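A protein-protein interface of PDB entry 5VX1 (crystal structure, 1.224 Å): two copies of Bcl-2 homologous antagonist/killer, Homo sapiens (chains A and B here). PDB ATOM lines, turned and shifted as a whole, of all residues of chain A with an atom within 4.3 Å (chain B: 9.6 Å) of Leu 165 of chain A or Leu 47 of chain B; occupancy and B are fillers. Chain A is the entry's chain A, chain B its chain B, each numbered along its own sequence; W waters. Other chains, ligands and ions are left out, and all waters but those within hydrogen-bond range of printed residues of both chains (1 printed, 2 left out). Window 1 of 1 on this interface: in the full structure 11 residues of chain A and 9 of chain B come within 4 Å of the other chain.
ND2 of Asn 166 of chain A lies close to NE2 of Gln 50 of chain B (3.3 Å).
The backbone NH (N) of Leu 167 of chain A is in hydrogen-bond range of the side-chain amide oxygen (OE1) of Gln 50 of chain B (2.9 Å).
The side-chain amide nitrogen (ND2) of Asn 166 of chain A sits at hydrogen-bond distance from the backbone carbonyl oxygen (O) of Ser 52 of chain B (2.7 Å).
OE1 of Gln 57 of chain A is in hydrogen-bond range of N of Leu 47 of chain B.
The side-chain amide nitrogen of Gln 57 of chain A sits at hydrogen-bond distance from the backbone carbonyl oxygen of Val 45 of chain B (2.9 Å).
O of Pro 42 of chain B lies within hydrogen-bond range of OG1 of Thr 46 of chain B (2.8 Å).
Among the printed residues, merely in contact across the chains: Thr 54 of chain A with Gln 28 of chain B (3.5 Å), Ala 163 of chain A with Ser 52 of chain B (3.6 Å), Gln 57 of chain A with Thr 46 of chain B (3.6 Å), Asn 166 of chain A with Pro 51 of chain B (3.7 Å), Val 162 of chain A with Pro 51 of chain B (3.7 Å), Thr 54 of chain A with Phe 24 of chain B (3.7 Å), Gln 57 of chain A with Phe 24 of chain B (3.8 Å), Thr 54 of chain A with Tyr 25 of chain B (3.8 Å) and Leu 165 of chain A with Leu 47 of chain B (3.9 Å).
Of the printed residues of chain B, Thr 54 of chain A touches Phe 24, Tyr 25 and Gln 28.
No residue of chain B comes within 4 Å of Val 58 of chain A.
No residue of chain B comes within 4 Å of Ala 164 of chain A.
Of chain B, only Leu 47 (3.9 Å) comes within 4 Å of Leu 165 of chain A.
Printed residues of chain A within 4 Å of Gln 28 of chain B: Thr 54 (3.5 Å).
Printed residues of chain A within 4 Å of Thr 46 of chain B: Gln 57.
Of chain A, only Gln 57 (3.0 Å) and Leu 165 (3.9 Å) come within 4 Å of Leu 47 of chain B.
The nearest printed residue of chain A that does not touch Leu 47 of chain B is Val 58 of chain A (4.1 Å).
Of the 11 printed residues of chain A, 7 touch a printed residue of chain B.
Printed residues of chain A that touch a printed residue of chain B: Thr 54, Gln 57, Val 162, Ala 163, Leu 165, Asn 166 and Leu 167.
Hydrophobic or aromatic side chains of chain A that line the printed part of chain B: Ala 163, Leu 165 and Leu 167.
Along chain A the printed residues that touch a printed residue of chain B span positions 54 to 167.
Printed residues of chain B that touch a printed residue of chain A: Phe 24, Tyr 25, Gln 28, Val 45, Thr 46, Leu 47, Gln 50, Pro 51 and Ser 52.
Hydrophobic or aromatic side chains of chain B that line the printed part of chain A: Phe 24, Tyr 25, Leu 47 and Pro 51.
Among the printed residues, 14 pairs touch across the chains.
Among the printed residues, no Asp or Glu carboxylate lies within 4 Å of a Lys or Arg side-chain nitrogen of the other chain.
No position is printed for both chains.
Water W1 lies within hydrogen-bond range of O of Ser 52 of chain B and ND2 of Asn 166 of chain A.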
ATOM      1  N   THR A  54       4.140 -29.393  27.576  1.00  0.00           N
ATOM      2  CA  THR A  54       3.347 -28.467  26.785  1.00  0.00           C
ATOM      3  C   THR A  54       1.863 -28.773  26.914  1.00  0.00           C
ATOM      4  O   THR A  54       1.040 -27.879  27.159  1.00  0.00           O
ATOM      5  CB  THR A  54       3.809 -28.543  25.336  1.00  0.00           C
ATOM      6  OG1 THR A  54       5.210 -28.330  25.290  1.00  0.00           O
ATOM      7  CG2 THR A  54       3.091 -27.497  24.507  1.00  0.00           C
ATOM      8  N   GLN A  57       0.377 -28.000  30.288  1.00  0.00           N
ATOM      9  CA  GLN A  57       0.084 -26.579  30.467  1.00  0.00           C
ATOM     10  C   GLN A  57      -1.127 -26.154  29.649  1.00  0.00           C
ATOM     11  O   GLN A  57      -1.922 -25.336  30.104  1.00  0.00           O
ATOM     12  CB  GLN A  57       1.306 -25.739  30.103  1.00  0.00           C
ATOM     13  CG  GLN A  57       2.494 -26.024  31.015  1.00  0.00           C
ATOM     14  CD  GLN A  57       3.574 -24.961  30.868  1.00  0.00           C
ATOM     15  OE1 GLN A  57       3.291 -23.756  30.758  1.00  0.00           O
ATOM     16  NE2 GLN A  57       4.809 -25.406  30.846  1.00  0.00           N
ATOM     17  N   VAL A  58      -1.315 -26.717  28.457  1.00  0.00           N
ATOM     18  CA  VAL A  58      -2.517 -26.381  27.705  1.00  0.00           C
ATOM     19  C   VAL A  58      -3.758 -26.792  28.509  1.00  0.00           C
ATOM     20  O   VAL A  58      -4.723 -26.025  28.650  1.00  0.00           O
ATOM     21  CB  VAL A  58      -2.492 -27.055  26.328  1.00  0.00           C
ATOM     22  CG1 VAL A  58      -3.830 -26.863  25.652  1.00  0.00           C
ATOM     23  CG2 VAL A  58      -1.438 -26.457  25.432  1.00  0.00           C
ATOM     24  N   GLN A  61      -4.376 -24.415  31.409  1.00  0.00           N
ATOM     25  CA  GLN A  61      -4.885 -23.096  31.049  1.00  0.00           C
ATOM     26  C   GLN A  61      -6.336 -23.167  30.581  1.00  0.00           C
ATOM     27  O   GLN A  61      -7.144 -22.286  30.894  1.00  0.00           O
ATOM     28  CB  GLN A  61      -3.976 -22.487  29.985  1.00  0.00           C
ATOM     29  CG  GLN A  61      -2.583 -22.190  30.480  1.00  0.00           C
ATOM     30  CD  GLN A  61      -2.605 -21.137  31.550  1.00  0.00           C
ATOM     31  OE1 GLN A  61      -2.220 -21.387  32.696  1.00  0.00           O
ATOM     32  NE2 GLN A  61      -3.108 -19.960  31.200  1.00  0.00           N
ATOM     33  N   LEU A  62      -6.697 -24.226  29.872  1.00  0.00           N
ATOM     34  CA  LEU A  62      -8.069 -24.355  29.401  1.00  0.00           C
ATOM     35  C   LEU A  62      -9.025 -24.573  30.553  1.00  0.00           C
ATOM     36  O   LEU A  62     -10.184 -24.138  30.504  1.00  0.00           O
ATOM     37  CB  LEU A  62      -8.164 -25.501  28.406  1.00  0.00           C
ATOM     38  CG  LEU A  62      -7.441 -25.238  27.076  1.00  0.00           C
ATOM     39  CD1 LEU A  62      -7.623 -26.478  26.195  1.00  0.00           C
ATOM     40  CD2 LEU A  62      -8.000 -24.000  26.367  1.00  0.00           C
ATOM     41  N   VAL A 162      -1.848 -26.282  21.108  1.00  0.00           N
ATOM     42  CA  VAL A 162      -1.404 -25.009  21.627  1.00  0.00           C
ATOM     43  C   VAL A 162      -2.215 -23.848  21.083  1.00  0.00           C
ATOM     44  O   VAL A 162      -2.279 -22.791  21.717  1.00  0.00           O
ATOM     45  CB  VAL A 162       0.104 -24.795  21.407  1.00  0.00           C
ATOM     46  CG1 VAL A 162       0.932 -25.755  22.279  1.00  0.00           C
ATOM     47  CG2 VAL A 162       0.485 -24.848  19.922  1.00  0.00           C
ATOM     48  N   ALA A 163      -2.803 -23.992  19.895  1.00  0.00           N
ATOM     49  CA  ALA A 163      -3.601 -22.908  19.345  1.00  0.00           C
ATOM     50  C   ALA A 163      -4.902 -22.656  20.099  1.00  0.00           C
ATOM     51  O   ALA A 163      -5.498 -21.582  19.925  1.00  0.00           O
ATOM     52  CB  ALA A 163      -3.886 -23.177  17.871  1.00  0.00           C
ATOM     53  N   ALA A 164      -5.303 -23.565  20.976  1.00  0.00           N
ATOM     54  CA  ALA A 164      -6.480 -23.328  21.798  1.00  0.00           C
ATOM     55  C   ALA A 164      -6.267 -22.174  22.761  1.00  0.00           C
ATOM     56  O   ALA A 164      -7.247 -21.620  23.275  1.00  0.00           O
ATOM     57  CB  ALA A 164      -6.805 -24.558  22.633  1.00  0.00           C
ATOM     58  N   LEU A 165      -5.014 -21.798  23.033  1.00  0.00           N
ATOM     59  CA  LEU A 165      -4.681 -20.750  23.994  1.00  0.00           C
ATOM     60  C   LEU A 165      -4.565 -19.369  23.370  1.00  0.00           C
ATOM     61  O   LEU A 165      -4.488 -18.378  24.105  1.00  0.00           O
ATOM     62  CB  LEU A 165      -3.345 -21.063  24.676  1.00  0.00           C
ATOM     63  CG  LEU A 165      -3.351 -22.377  25.441  1.00  0.00           C
ATOM     64  CD1 LEU A 165      -2.119 -22.491  26.319  1.00  0.00           C
ATOM     65  CD2 LEU A 165      -4.635 -22.501  26.282  1.00  0.00           C
ATOM     66  N   ASN A 166      -4.514 -19.281  22.045  1.00  0.00           N
ATOM     67  CA  ASN A 166      -4.442 -17.987  21.379  1.00  0.00           C
ATOM     68  C   ASN A 166      -5.687 -17.157  21.660  1.00  0.00           C
ATOM     69  O   ASN A 166      -6.789 -17.684  21.848  1.00  0.00           O
ATOM     70  CB  ASN A 166      -4.287 -18.183  19.873  1.00  0.00           C
ATOM     71  CG  ASN A 166      -2.848 -18.325  19.465  1.00  0.00           C
ATOM     72  OD1 ASN A 166      -1.962 -18.401  20.317  1.00  0.00           O
ATOM     73  ND2 ASN A 166      -2.595 -18.367  18.162  1.00  0.00           N
ATOM     74  N   LEU A 167      -5.499 -15.839  21.669  1.00  0.00           N
ATOM     75  CA  LEU A 167      -6.579 -14.896  21.914  1.00  0.00           C
ATOM     76  C   LEU A 167      -7.714 -15.063  20.905  1.00  0.00           C
ATOM     77  O   LEU A 167      -7.553 -14.758  19.725  1.00  0.00           O
ATOM     78  CB  LEU A 167      -6.039 -13.473  21.834  1.00  0.00           C
ATOM     79  CG  LEU A 167      -6.840 -12.497  22.685  1.00  0.00           C
ATOM     80  CD1 LEU A 167      -6.386 -12.587  24.143  1.00  0.00           C
ATOM     81  CD2 LEU A 167      -6.712 -11.080  22.144  1.00  0.00           C
ATOM     82  N   ARG B  20      12.161 -16.681  22.377  1.00  0.00           N
ATOM     83  CA  ARG B  20      11.435 -17.097  23.571  1.00  0.00           C
ATOM     84  C   ARG B  20      10.805 -18.469  23.380  1.00  0.00           C
ATOM     85  O   ARG B  20      10.768 -19.261  24.313  1.00  0.00           O
ATOM     86  CB  ARG B  20      10.402 -16.025  23.913  1.00  0.00           C
ATOM     87  CG  ARG B  20      11.054 -14.794  24.558  1.00  0.00           C
ATOM     88  CD  ARG B  20      10.057 -13.686  24.891  1.00  0.00           C
ATOM     89  NE  ARG B  20      10.705 -12.607  25.644  1.00  0.00           N
ATOM     90  CZ  ARG B  20      11.015 -12.670  26.936  1.00  0.00           C
ATOM     91  NH1 ARG B  20      10.706 -13.749  27.655  1.00  0.00           N
ATOM     92  NH2 ARG B  20      11.616 -11.639  27.522  1.00  0.00           N
ATOM     93  N   SER B  21      10.302 -18.763  22.197  1.00  0.00           N
ATOM     94  CA  SER B  21       9.793 -20.107  21.950  1.00  0.00           C
ATOM     95  C   SER B  21      10.925 -21.134  21.959  1.00  0.00           C
ATOM     96  O   SER B  21      10.785 -22.214  22.534  1.00  0.00           O
ATOM     97  CB  SER B  21       9.056 -20.128  20.606  1.00  0.00           C
ATOM     98  OG  SER B  21       8.573 -21.426  20.329  1.00  0.00           O
ATOM     99  N   VAL B  23      13.724 -21.018  23.622  1.00  0.00           N
ATOM    100  CA  VAL B  23      14.111 -21.256  25.017  1.00  0.00           C
ATOM    101  C   VAL B  23      13.142 -22.214  25.698  1.00  0.00           C
ATOM    102  O   VAL B  23      13.543 -23.132  26.427  1.00  0.00           O
ATOM    103  CB  VAL B  23      14.207 -19.918  25.768  1.00  0.00           C
ATOM    104  CG1 VAL B  23      14.221 -20.121  27.272  1.00  0.00           C
ATOM    105  CG2 VAL B  23      15.442 -19.147  25.285  1.00  0.00           C
ATOM    106  N   PHE B  24      11.844 -21.954  25.565  1.00  0.00           N
ATOM    107  CA  PHE B  24      10.850 -22.839  26.186  1.00  0.00           C
ATOM    108  C   PHE B  24      11.049 -24.300  25.773  1.00  0.00           C
ATOM    109  O   PHE B  24      11.124 -25.212  26.603  1.00  0.00           O
ATOM    110  CB  PHE B  24       9.440 -22.375  25.804  1.00  0.00           C
ATOM    111  CG  PHE B  24       8.355 -23.267  26.315  1.00  0.00           C
ATOM    112  CD1 PHE B  24       7.935 -23.153  27.606  1.00  0.00           C
ATOM    113  CD2 PHE B  24       7.776 -24.212  25.497  1.00  0.00           C
ATOM    114  CE1 PHE B  24       6.937 -23.991  28.086  1.00  0.00           C
ATOM    115  CE2 PHE B  24       6.784 -25.056  25.964  1.00  0.00           C
ATOM    116  CZ  PHE B  24       6.379 -24.938  27.258  1.00  0.00           C
ATOM    117  N   TYR B  25      11.196 -24.523  24.459  1.00  0.00           N
ATOM    118  CA  TYR B  25      11.291 -25.889  23.956  1.00  0.00           C
ATOM    119  C   TYR B  25      12.668 -26.485  24.211  1.00  0.00           C
ATOM    120  O   TYR B  25      12.747 -27.694  24.484  1.00  0.00           O
ATOM    121  CB  TYR B  25      10.885 -25.973  22.469  1.00  0.00           C
ATOM    122  CG  TYR B  25       9.391 -25.811  22.250  1.00  0.00           C
ATOM    123  CD1 TYR B  25       8.515 -26.843  22.568  1.00  0.00           C
ATOM    124  CD2 TYR B  25       8.850 -24.623  21.761  1.00  0.00           C
ATOM    125  CE1 TYR B  25       7.147 -26.706  22.392  1.00  0.00           C
ATOM    126  CE2 TYR B  25       7.485 -24.479  21.583  1.00  0.00           C
ATOM    127  CZ  TYR B  25       6.636 -25.519  21.904  1.00  0.00           C
ATOM    128  OH  TYR B  25       5.271 -25.389  21.723  1.00  0.00           O
ATOM    129  N   GLN B  28      12.349 -27.508  27.919  1.00  0.00           N
ATOM    130  CA  GLN B  28      11.496 -28.688  28.071  1.00  0.00           C
ATOM    131  C   GLN B  28      12.262 -29.985  27.843  1.00  0.00           C
ATOM    132  O   GLN B  28      11.822 -31.041  28.326  1.00  0.00           O
ATOM    133  CB  GLN B  28      10.314 -28.688  27.090  1.00  0.00           C
ATOM    134  CG  GLN B  28       9.151 -27.724  27.360  1.00  0.00           C
ATOM    135  CD  GLN B  28       8.292 -28.087  28.573  1.00  0.00           C
ATOM    136  OE1 GLN B  28       7.499 -29.039  28.537  1.00  0.00           O
ATOM    137  NE2 GLN B  28       8.436 -27.313  29.651  1.00  0.00           N
ATOM    138  N   ASP B  41      13.742 -21.146  36.210  1.00  0.00           N
ATOM    139  CA  ASP B  41      13.280 -19.807  35.925  1.00  0.00           C
ATOM    140  C   ASP B  41      11.851 -19.901  35.392  1.00  0.00           C
ATOM    141  O   ASP B  41      11.626 -20.533  34.339  1.00  0.00           O
ATOM    142  CB  ASP B  41      14.176 -19.252  34.825  1.00  0.00           C
ATOM    143  CG  ASP B  41      13.853 -17.821  34.456  1.00  0.00           C
ATOM    144  OD1 ASP B  41      12.764 -17.355  34.854  1.00  0.00           O
ATOM    145  OD2 ASP B  41      14.636 -17.205  33.694  1.00  0.00           O
ATOM    146  N   PRO B  42      10.844 -19.346  36.085  1.00  0.00           N
ATOM    147  CA  PRO B  42       9.457 -19.458  35.598  1.00  0.00           C
ATOM    148  C   PRO B  42       9.305 -18.982  34.177  1.00  0.00           C
ATOM    149  O   PRO B  42       8.466 -19.525  33.440  1.00  0.00           O
ATOM    150  CB  PRO B  42       8.648 -18.578  36.571  1.00  0.00           C
ATOM    151  CG  PRO B  42       9.569 -18.298  37.734  1.00  0.00           C
ATOM    152  CD  PRO B  42      10.982 -18.527  37.302  1.00  0.00           C
ATOM    153  N   GLU B  43      10.093 -17.987  33.767  1.00  0.00           N
ATOM    154  CA  GLU B  43       9.928 -17.469  32.433  1.00  0.00           C
ATOM    155  C   GLU B  43      10.372 -18.475  31.403  1.00  0.00           C
ATOM    156  O   GLU B  43       9.927 -18.407  30.253  1.00  0.00           O
ATOM    157  CB  GLU B  43      10.759 -16.216  32.300  1.00  0.00           C
ATOM    158  CG  GLU B  43       9.979 -15.027  31.962  1.00  0.00           C
ATOM    159  CD  GLU B  43      10.871 -13.835  31.674  1.00  0.00           C
ATOM    160  OE1 GLU B  43      10.779 -13.255  30.566  1.00  0.00           O
ATOM    161  OE2 GLU B  43      11.656 -13.487  32.554  1.00  0.00           O
ATOM    162  N   MET B  44      11.281 -19.374  31.777  1.00  0.00           N
ATOM    163  CA  MET B  44      11.719 -20.456  30.893  1.00  0.00           C
ATOM    164  C   MET B  44      10.672 -21.538  30.779  1.00  0.00           C
ATOM    165  O   MET B  44      10.415 -22.050  29.682  1.00  0.00           O
ATOM    166  CB  MET B  44      12.998 -21.086  31.430  1.00  0.00           C
ATOM    167  CG  MET B  44      14.179 -20.188  31.222  1.00  0.00           C
ATOM    168  SD  MET B  44      15.775 -21.007  31.312  1.00  0.00           S
ATOM    169  CE  MET B  44      16.759 -19.634  30.747  1.00  0.00           C
ATOM    170  N   VAL B  45      10.050 -21.890  31.901  1.00  0.00           N
ATOM    171  CA  VAL B  45       9.237 -23.102  31.999  1.00  0.00           C
ATOM    172  C   VAL B  45       7.763 -22.864  31.749  1.00  0.00           C
ATOM    173  O   VAL B  45       6.982 -23.816  31.862  1.00  0.00           O
ATOM    174  CB  VAL B  45       9.394 -23.822  33.356  1.00  0.00           C
ATOM    175  CG1 VAL B  45      10.745 -24.327  33.525  1.00  0.00           C
ATOM    176  CG2 VAL B  45       9.020 -22.930  34.533  1.00  0.00           C
ATOM    177  N   THR B  46       7.353 -21.639  31.445  1.00  0.00           N
ATOM    178  CA  THR B  46       5.959 -21.316  31.200  1.00  0.00           C
ATOM    179  C   THR B  46       5.745 -21.090  29.710  1.00  0.00           C
ATOM    180  O   THR B  46       6.492 -20.340  29.076  1.00  0.00           O
ATOM    181  CB  THR B  46       5.576 -20.060  31.986  1.00  0.00           C
ATOM    182  OG1 THR B  46       5.787 -20.312  33.380  1.00  0.00           O
ATOM    183  CG2 THR B  46       4.129 -19.740  31.791  1.00  0.00           C
ATOM    184  N   LEU B  47       4.714 -21.726  29.159  1.00  0.00           N
ATOM    185  CA  LEU B  47       4.439 -21.560  27.737  1.00  0.00           C
ATOM    186  C   LEU B  47       4.279 -20.082  27.416  1.00  0.00           C
ATOM    187  O   LEU B  47       3.544 -19.380  28.121  1.00  0.00           O
ATOM    188  CB  LEU B  47       3.099 -22.243  27.452  1.00  0.00           C
ATOM    189  CG  LEU B  47       2.972 -23.533  26.653  1.00  0.00           C
ATOM    190  CD1 LEU B  47       1.517 -23.763  26.391  1.00  0.00           C
ATOM    191  CD2 LEU B  47       3.688 -23.490  25.359  1.00  0.00           C
ATOM    192  N   PRO B  48       4.911 -19.574  26.351  1.00  0.00           N
ATOM    193  CA  PRO B  48       4.754 -18.156  26.010  1.00  0.00           C
ATOM    194  C   PRO B  48       3.322 -17.854  25.600  1.00  0.00           C
ATOM    195  O   PRO B  48       2.536 -18.742  25.259  1.00  0.00           O
ATOM    196  CB  PRO B  48       5.702 -17.961  24.819  1.00  0.00           C
ATOM    197  CG  PRO B  48       6.596 -19.167  24.816  1.00  0.00           C
ATOM    198  CD  PRO B  48       5.783 -20.278  25.393  1.00  0.00           C
ATOM    199  N   LEU B  49       2.982 -16.571  25.629  1.00  0.00           N
ATOM    200  CA  LEU B  49       1.711 -16.177  25.044  1.00  0.00           C
ATOM    201  C   LEU B  49       1.760 -16.340  23.530  1.00  0.00           C
ATOM    202  O   LEU B  49       2.832 -16.341  22.911  1.00  0.00           O
ATOM    203  CB  LEU B  49       1.367 -14.741  25.406  1.00  0.00           C
ATOM    204  CG  LEU B  49       1.183 -14.553  26.906  1.00  0.00           C
ATOM    205  CD1 LEU B  49       0.457 -13.254  27.169  1.00  0.00           C
ATOM    206  CD2 LEU B  49       0.425 -15.735  27.504  1.00  0.00           C
ATOM    207  N   GLN B  50       0.578 -16.480  22.939  1.00  0.00           N
ATOM    208  CA  GLN B  50       0.396 -16.830  21.532  1.00  0.00           C
ATOM    209  C   GLN B  50       1.342 -17.957  21.099  1.00  0.00           C
ATOM    210  O   GLN B  50       2.099 -17.809  20.135  1.00  0.00           O
ATOM    211  CB  GLN B  50       0.531 -15.610  20.625  1.00  0.00           C
ATOM    212  CG  GLN B  50      -0.505 -14.521  20.891  1.00  0.00           C
ATOM    213  CD  GLN B  50      -1.916 -14.894  20.442  1.00  0.00           C
ATOM    214  OE1 GLN B  50      -2.869 -14.809  21.220  1.00  0.00           O
ATOM    215  NE2 GLN B  50      -2.059 -15.278  19.175  1.00  0.00           N
ATOM    216  N   PRO B  51       1.315 -19.102  21.793  1.00  0.00           N
ATOM    217  CA  PRO B  51       2.272 -20.168  21.467  1.00  0.00           C
ATOM    218  C   PRO B  51       2.120 -20.758  20.073  1.00  0.00           C
ATOM    219  O   PRO B  51       3.040 -21.439  19.600  1.00  0.00           O
ATOM    220  CB  PRO B  51       2.036 -21.207  22.578  1.00  0.00           C
ATOM    221  CG  PRO B  51       0.619 -20.959  23.039  1.00  0.00           C
ATOM    222  CD  PRO B  51       0.406 -19.480  22.898  1.00  0.00           C
ATOM    223  N   SER B  52       0.947 -20.579  19.488  1.00  0.00           N
ATOM    224  CA  SER B  52       0.705 -20.893  18.107  1.00  0.00           C
ATOM    225  C   SER B  52       0.850 -19.581  17.361  1.00  0.00           C
ATOM    226  O   SER B  52      -0.073 -18.782  17.233  1.00  0.00           O
ATOM    227  CB  SER B  52      -0.667 -21.492  17.900  1.00  0.00           C
ATOM    228  OG  SER B  52      -0.678 -22.183  16.687  1.00  0.00           O
ATOM    229  N   SER B  53       2.044 -19.354  16.904  1.00  0.00           N
ATOM    230  CA  SER B  53       2.255 -18.466  15.791  1.00  0.00           C
ATOM    231  C   SER B  53       3.319 -19.082  14.906  1.00  0.00           C
ATOM    232  O   SER B  53       4.028 -20.008  15.299  1.00  0.00           O
ATOM    233  CB  SER B  53       2.761 -17.134  16.309  1.00  0.00           C
ATOM    234  OG  SER B  53       4.043 -17.311  16.890  1.00  0.00           O
ATOM    235  N   GLY B  56       6.514 -18.720  16.822  1.00  0.00           N
ATOM    236  CA  GLY B  56       6.609 -19.728  17.856  1.00  0.00           C
ATOM    237  C   GLY B  56       6.974 -21.079  17.270  1.00  0.00           C
ATOM    238  O   GLY B  56       7.779 -21.821  17.843  1.00  0.00           O
ATOM    239  N   ARG B  60      10.271 -23.496  17.976  1.00  0.00           N
ATOM    240  CA  ARG B  60      10.107 -24.880  18.391  1.00  0.00           C
ATOM    241  C   ARG B  60      10.939 -25.824  17.527  1.00  0.00           C
ATOM    242  O   ARG B  60      11.669 -26.686  18.037  1.00  0.00           O
ATOM    243  CB  ARG B  60       8.628 -25.250  18.335  1.00  0.00           C
ATOM    244  CG  ARG B  60       8.455 -26.673  18.731  1.00  0.00           C
ATOM    245  CD  ARG B  60       7.069 -27.212  18.505  1.00  0.00           C
ATOM    246  NE  ARG B  60       7.027 -28.525  19.138  1.00  0.00           N
ATOM    247  CZ  ARG B  60       6.379 -29.579  18.669  1.00  0.00           C
ATOM    248  NH1 ARG B  60       5.698 -29.492  17.535  1.00  0.00           N
ATOM    249  NH2 ARG B  60       6.428 -30.722  19.339  1.00  0.00           N
HETATM  250  O   HOH W   1      -0.548 -16.580  16.025  1.00  0.00           O
